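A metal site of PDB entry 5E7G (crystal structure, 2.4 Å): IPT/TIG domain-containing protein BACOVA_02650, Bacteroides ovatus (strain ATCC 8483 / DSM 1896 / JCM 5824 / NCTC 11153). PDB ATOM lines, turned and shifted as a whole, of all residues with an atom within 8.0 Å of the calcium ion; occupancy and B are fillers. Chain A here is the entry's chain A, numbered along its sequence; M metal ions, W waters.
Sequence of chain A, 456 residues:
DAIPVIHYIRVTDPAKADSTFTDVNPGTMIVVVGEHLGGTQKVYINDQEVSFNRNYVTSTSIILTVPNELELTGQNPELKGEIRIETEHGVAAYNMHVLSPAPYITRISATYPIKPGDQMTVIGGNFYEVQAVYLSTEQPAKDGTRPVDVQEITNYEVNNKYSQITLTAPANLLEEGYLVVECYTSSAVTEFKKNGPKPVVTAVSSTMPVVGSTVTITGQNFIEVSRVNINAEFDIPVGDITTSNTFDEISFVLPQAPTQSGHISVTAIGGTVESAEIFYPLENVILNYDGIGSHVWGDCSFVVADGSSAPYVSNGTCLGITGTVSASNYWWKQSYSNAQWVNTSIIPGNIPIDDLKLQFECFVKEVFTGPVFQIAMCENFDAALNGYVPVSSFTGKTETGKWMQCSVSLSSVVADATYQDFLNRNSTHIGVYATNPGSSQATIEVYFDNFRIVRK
The backbone NH (N) of Ile 292 is in hydrogen-bond range of the side-chain amide oxygen (OD1) of Asn 288 (3.1 Å).
The side-chain carboxylate (OD1) of Asp 449 sits close to the side-chain amide oxygen (OD1) of Asn 450, 3.5 Å away.
The calcium ion is bound by the side-chain carboxylate (OD2) of Asp 449 (2.4 Å), the side-chain carboxylate (OD2) of Asp 290 (2.4 Å), the backbone carbonyl oxygen (O) of Thr 317 (2.4 Å), the side-chain carboxylate (OD1) of Asp 449 (2.4 Å), water W1 (2.4 Å), the backbone carbonyl oxygen (O) of Asn 288 (2.4 Å) and the backbone carbonyl oxygen (O) of Asn 315 (2.4 Å).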
ATOM      1  N   VAL A 210     -16.443 -30.107  -1.948  1.00  0.00           N
ATOM      2  CA  VAL A 210     -17.817 -30.260  -1.519  1.00  0.00           C
ATOM      3  C   VAL A 210     -17.859 -30.499  -0.005  1.00  0.00           C
ATOM      4  O   VAL A 210     -17.025 -31.225   0.533  1.00  0.00           O
ATOM      5  CB  VAL A 210     -18.485 -31.427  -2.294  1.00  0.00           C
ATOM      6  CG1 VAL A 210     -19.915 -31.650  -1.839  1.00  0.00           C
ATOM      7  CG2 VAL A 210     -18.430 -31.148  -3.817  1.00  0.00           C
ATOM      8  N   VAL A 285     -17.212 -18.067  -9.001  1.00  0.00           N
ATOM      9  CA  VAL A 285     -18.146 -19.076  -9.476  1.00  0.00           C
ATOM     10  C   VAL A 285     -19.001 -18.492 -10.583  1.00  0.00           C
ATOM     11  O   VAL A 285     -19.432 -17.350 -10.490  1.00  0.00           O
ATOM     12  CB  VAL A 285     -19.043 -19.595  -8.327  1.00  0.00           C
ATOM     13  CG1 VAL A 285     -20.091 -20.584  -8.836  1.00  0.00           C
ATOM     14  CG2 VAL A 285     -18.190 -20.223  -7.232  1.00  0.00           C
ATOM     15  N   LEU A 287     -21.325 -20.921 -12.371  1.00  0.00           N
ATOM     16  CA  LEU A 287     -22.491 -21.801 -12.440  1.00  0.00           C
ATOM     17  C   LEU A 287     -22.459 -22.857 -11.309  1.00  0.00           C
ATOM     18  O   LEU A 287     -21.514 -23.644 -11.200  1.00  0.00           O
ATOM     19  CB  LEU A 287     -22.539 -22.493 -13.815  1.00  0.00           C
ATOM     20  CG  LEU A 287     -23.746 -23.389 -14.109  1.00  0.00           C
ATOM     21  CD1 LEU A 287     -25.041 -22.601 -14.067  1.00  0.00           C
ATOM     22  CD2 LEU A 287     -23.597 -24.098 -15.442  1.00  0.00           C
ATOM     23  N   ASN A 288     -23.488 -22.853 -10.464  1.00  0.00           N
ATOM     24  CA  ASN A 288     -23.571 -23.791  -9.352  1.00  0.00           C
ATOM     25  C   ASN A 288     -24.963 -24.377  -9.189  1.00  0.00           C
ATOM     26  O   ASN A 288     -25.209 -25.187  -8.299  1.00  0.00           O
ATOM     27  CB  ASN A 288     -23.125 -23.127  -8.053  1.00  0.00           C
ATOM     28  CG  ASN A 288     -24.016 -21.972  -7.630  1.00  0.00           C
ATOM     29  OD1 ASN A 288     -25.100 -21.763  -8.198  1.00  0.00           O
ATOM     30  ND2 ASN A 288     -23.584 -21.231  -6.631  1.00  0.00           N
ATOM     31  N   TYR A 289     -25.889 -23.962 -10.066  1.00  0.00           N
ATOM     32  CA  TYR A 289     -27.268 -24.465 -10.045  1.00  0.00           C
ATOM     33  C   TYR A 289     -27.970 -24.132  -8.726  1.00  0.00           C
ATOM     34  O   TYR A 289     -28.983 -24.749  -8.398  1.00  0.00           O
ATOM     35  CB  TYR A 289     -27.292 -25.976 -10.312  1.00  0.00           C
ATOM     36  CG  TYR A 289     -26.401 -26.383 -11.466  1.00  0.00           C
ATOM     37  CD1 TYR A 289     -26.753 -26.094 -12.770  1.00  0.00           C
ATOM     38  CD2 TYR A 289     -25.205 -27.050 -11.246  1.00  0.00           C
ATOM     39  CE1 TYR A 289     -25.940 -26.462 -13.827  1.00  0.00           C
ATOM     40  CE2 TYR A 289     -24.386 -27.428 -12.293  1.00  0.00           C
ATOM     41  CZ  TYR A 289     -24.762 -27.137 -13.582  1.00  0.00           C
ATOM     42  OH  TYR A 289     -23.934 -27.516 -14.615  1.00  0.00           O
ATOM     43  N   ASP A 290     -27.442 -23.148  -8.004  1.00  0.00           N
ATOM     44  CA  ASP A 290     -27.991 -22.740  -6.719  1.00  0.00           C
ATOM     45  C   ASP A 290     -28.098 -21.217  -6.650  1.00  0.00           C
ATOM     46  O   ASP A 290     -27.890 -20.628  -5.588  1.00  0.00           O
ATOM     47  CB  ASP A 290     -27.112 -23.260  -5.569  1.00  0.00           C
ATOM     48  CG  ASP A 290     -27.039 -24.767  -5.524  1.00  0.00           C
ATOM     49  OD1 ASP A 290     -28.116 -25.390  -5.509  1.00  0.00           O
ATOM     50  OD2 ASP A 290     -25.918 -25.332  -5.518  1.00  0.00           O
ATOM     51  N   GLY A 291     -28.404 -20.579  -7.780  1.00  0.00           N
ATOM     52  CA  GLY A 291     -28.583 -19.127  -7.800  1.00  0.00           C
ATOM     53  C   GLY A 291     -27.526 -18.380  -8.603  1.00  0.00           C
ATOM     54  O   GLY A 291     -27.773 -17.243  -9.013  1.00  0.00           O
ATOM     55  N   ILE A 292     -26.359 -18.987  -8.779  1.00  0.00           N
ATOM     56  CA  ILE A 292     -25.352 -18.451  -9.698  1.00  0.00           C
ATOM     57  C   ILE A 292     -25.494 -19.122 -11.050  1.00  0.00           C
ATOM     58  O   ILE A 292     -25.206 -20.312 -11.175  1.00  0.00           O
ATOM     59  CB  ILE A 292     -23.914 -18.681  -9.183  1.00  0.00           C
ATOM     60  CG1 ILE A 292     -23.748 -18.175  -7.753  1.00  0.00           C
ATOM     61  CG2 ILE A 292     -22.924 -18.000 -10.105  1.00  0.00           C
ATOM     62  CD1 ILE A 292     -24.084 -16.729  -7.573  1.00  0.00           C
ATOM     63  N   VAL A 303     -29.682 -33.105  -9.324  1.00  0.00           N
ATOM     64  CA  VAL A 303     -29.828 -33.883  -8.106  1.00  0.00           C
ATOM     65  C   VAL A 303     -29.327 -33.099  -6.902  1.00  0.00           C
ATOM     66  O   VAL A 303     -28.368 -32.332  -7.007  1.00  0.00           O
ATOM     67  CB  VAL A 303     -29.046 -35.218  -8.200  1.00  0.00           C
ATOM     68  CG1 VAL A 303     -29.243 -36.059  -6.950  1.00  0.00           C
ATOM     69  CG2 VAL A 303     -29.480 -35.992  -9.431  1.00  0.00           C
ATOM     70  N   SER A 314     -23.235 -33.182  -1.784  1.00  0.00           N
ATOM     71  CA  SER A 314     -23.233 -32.134  -2.800  1.00  0.00           C
ATOM     72  C   SER A 314     -23.459 -30.763  -2.189  1.00  0.00           C
ATOM     73  O   SER A 314     -24.135 -30.618  -1.172  1.00  0.00           O
ATOM     74  CB  SER A 314     -24.312 -32.401  -3.850  1.00  0.00           C
ATOM     75  OG  SER A 314     -25.619 -32.199  -3.330  1.00  0.00           O
ATOM     76  N   ASN A 315     -22.887 -29.733  -2.829  1.00  0.00           N
ATOM     77  CA  ASN A 315     -23.217 -28.355  -2.504  1.00  0.00           C
ATOM     78  C   ASN A 315     -24.487 -27.910  -3.236  1.00  0.00           C
ATOM     79  O   ASN A 315     -24.447 -27.455  -4.376  1.00  0.00           O
ATOM     80  CB  ASN A 315     -22.061 -27.427  -2.866  1.00  0.00           C
ATOM     81  CG  ASN A 315     -20.900 -27.538  -1.897  1.00  0.00           C
ATOM     82  OD1 ASN A 315     -20.857 -28.435  -1.048  1.00  0.00           O
ATOM     83  ND2 ASN A 315     -19.939 -26.636  -2.038  1.00  0.00           N
ATOM     84  N   GLY A 316     -25.625 -28.071  -2.565  1.00  0.00           N
ATOM     85  CA  GLY A 316     -26.905 -27.783  -3.168  1.00  0.00           C
ATOM     86  C   GLY A 316     -27.178 -28.707  -4.333  1.00  0.00           C
ATOM     87  O   GLY A 316     -26.900 -29.913  -4.279  1.00  0.00           O
ATOM     88  N   THR A 317     -27.733 -28.144  -5.395  1.00  0.00           N
ATOM     89  CA  THR A 317     -28.026 -28.912  -6.594  1.00  0.00           C
ATOM     90  C   THR A 317     -26.780 -29.025  -7.471  1.00  0.00           C
ATOM     91  O   THR A 317     -25.946 -28.125  -7.496  1.00  0.00           O
ATOM     92  CB  THR A 317     -29.179 -28.280  -7.374  1.00  0.00           C
ATOM     93  OG1 THR A 317     -30.390 -28.414  -6.611  1.00  0.00           O
ATOM     94  CG2 THR A 317     -29.370 -28.938  -8.762  1.00  0.00           C
ATOM     95  N   CYS A 318     -26.663 -30.141  -8.182  1.00  0.00           N
ATOM     96  CA  CYS A 318     -25.552 -30.367  -9.099  1.00  0.00           C
ATOM     97  C   CYS A 318     -26.067 -31.064 -10.358  1.00  0.00           C
ATOM     98  O   CYS A 318     -27.086 -31.745 -10.327  1.00  0.00           O
ATOM     99  CB  CYS A 318     -24.456 -31.204  -8.422  1.00  0.00           C
ATOM    100  SG  CYS A 318     -24.925 -32.894  -8.049  1.00  0.00           S
ATOM    101  N   LEU A 319     -25.349 -30.857 -11.462  1.00  0.00           N
ATOM    102  CA  LEU A 319     -25.723 -31.419 -12.752  1.00  0.00           C
ATOM    103  C   LEU A 319     -25.386 -32.890 -12.825  1.00  0.00           C
ATOM    104  O   LEU A 319     -24.320 -33.302 -12.392  1.00  0.00           O
ATOM    105  CB  LEU A 319     -24.995 -30.676 -13.896  1.00  0.00           C
ATOM    106  CG  LEU A 319     -24.994 -31.327 -15.290  1.00  0.00           C
ATOM    107  CD1 LEU A 319     -26.380 -31.315 -15.898  1.00  0.00           C
ATOM    108  CD2 LEU A 319     -23.995 -30.607 -16.177  1.00  0.00           C
ATOM    109  N   TRP A 403     -15.637 -36.990  -5.162  1.00  0.00           N
ATOM    110  CA  TRP A 403     -15.507 -35.754  -5.901  1.00  0.00           C
ATOM    111  C   TRP A 403     -14.043 -35.454  -6.208  1.00  0.00           C
ATOM    112  O   TRP A 403     -13.156 -35.832  -5.446  1.00  0.00           O
ATOM    113  CB  TRP A 403     -16.130 -34.597  -5.124  1.00  0.00           C
ATOM    114  CG  TRP A 403     -17.648 -34.592  -5.120  1.00  0.00           C
ATOM    115  CD1 TRP A 403     -18.468 -35.126  -4.176  1.00  0.00           C
ATOM    116  CD2 TRP A 403     -18.503 -34.016  -6.124  1.00  0.00           C
ATOM    117  NE1 TRP A 403     -19.785 -34.927  -4.518  1.00  0.00           N
ATOM    118  CE2 TRP A 403     -19.832 -34.252  -5.708  1.00  0.00           C
ATOM    119  CE3 TRP A 403     -18.280 -33.342  -7.331  1.00  0.00           C
ATOM    120  CZ2 TRP A 403     -20.938 -33.829  -6.460  1.00  0.00           C
ATOM    121  CZ3 TRP A 403     -19.373 -32.917  -8.077  1.00  0.00           C
ATOM    122  CH2 TRP A 403     -20.688 -33.165  -7.638  1.00  0.00           C
ATOM    123  N   PHE A 448     -21.545 -32.821 -12.021  1.00  0.00           N
ATOM    124  CA  PHE A 448     -20.783 -31.586 -12.137  1.00  0.00           C
ATOM    125  C   PHE A 448     -21.329 -30.498 -11.213  1.00  0.00           C
ATOM    126  O   PHE A 448     -22.541 -30.392 -11.039  1.00  0.00           O
ATOM    127  CB  PHE A 448     -20.819 -31.040 -13.569  1.00  0.00           C
ATOM    128  CG  PHE A 448     -20.201 -31.944 -14.596  1.00  0.00           C
ATOM    129  CD1 PHE A 448     -20.981 -32.856 -15.283  1.00  0.00           C
ATOM    130  CD2 PHE A 448     -18.861 -31.852 -14.916  1.00  0.00           C
ATOM    131  CE1 PHE A 448     -20.425 -33.683 -16.259  1.00  0.00           C
ATOM    132  CE2 PHE A 448     -18.296 -32.680 -15.877  1.00  0.00           C
ATOM    133  CZ  PHE A 448     -19.083 -33.585 -16.551  1.00  0.00           C
ATOM    134  N   ASP A 449     -20.442 -29.657 -10.676  1.00  0.00           N
ATOM    135  CA  ASP A 449     -20.885 -28.527  -9.869  1.00  0.00           C
ATOM    136  C   ASP A 449     -19.788 -27.465  -9.757  1.00  0.00           C
ATOM    137  O   ASP A 449     -18.616 -27.755  -9.945  1.00  0.00           O
ATOM    138  CB  ASP A 449     -21.302 -29.015  -8.474  1.00  0.00           C
ATOM    139  CG  ASP A 449     -22.376 -28.136  -7.812  1.00  0.00           C
ATOM    140  OD1 ASP A 449     -22.571 -26.975  -8.238  1.00  0.00           O
ATOM    141  OD2 ASP A 449     -23.022 -28.609  -6.841  1.00  0.00           O
ATOM    142  N   ASN A 450     -20.202 -26.247  -9.428  1.00  0.00           N
ATOM    143  CA  ASN A 450     -19.276 -25.171  -9.076  1.00  0.00           C
ATOM    144  C   ASN A 450     -18.264 -24.804 -10.176  1.00  0.00           C
ATOM    145  O   ASN A 450     -17.056 -24.668  -9.917  1.00  0.00           O
ATOM    146  CB  ASN A 450     -18.537 -25.516  -7.782  1.00  0.00           C
ATOM    147  CG  ASN A 450     -19.466 -25.557  -6.578  1.00  0.00           C
ATOM    148  OD1 ASN A 450     -20.450 -24.814  -6.523  1.00  0.00           O
ATOM    149  ND2 ASN A 450     -19.170 -26.426  -5.606  1.00  0.00           N
ATOM    150  N   PHE A 451     -18.758 -24.625 -11.390  1.00  0.00           N
ATOM    151  CA  PHE A 451     -17.925 -24.105 -12.455  1.00  0.00           C
ATOM    152  C   PHE A 451     -17.438 -22.737 -12.025  1.00  0.00           C
ATOM    153  O   PHE A 451     -18.203 -21.909 -11.545  1.00  0.00           O
ATOM    154  CB  PHE A 451     -18.701 -24.017 -13.776  1.00  0.00           C
ATOM    155  CG  PHE A 451     -19.072 -25.364 -14.341  1.00  0.00           C
ATOM    156  CD1 PHE A 451     -18.230 -25.995 -15.225  1.00  0.00           C
ATOM    157  CD2 PHE A 451     -20.264 -25.982 -13.987  1.00  0.00           C
ATOM    158  CE1 PHE A 451     -18.557 -27.225 -15.761  1.00  0.00           C
ATOM    159  CE2 PHE A 451     -20.602 -27.212 -14.515  1.00  0.00           C
ATOM    160  CZ  PHE A 451     -19.745 -27.839 -15.415  1.00  0.00           C
HETATM  161 CA    CA M   1     -24.302 -26.648  -6.638  1.00  0.00          CA
HETATM  162  O   HOH W   1     -22.727 -25.255  -5.518  1.00  0.00           O
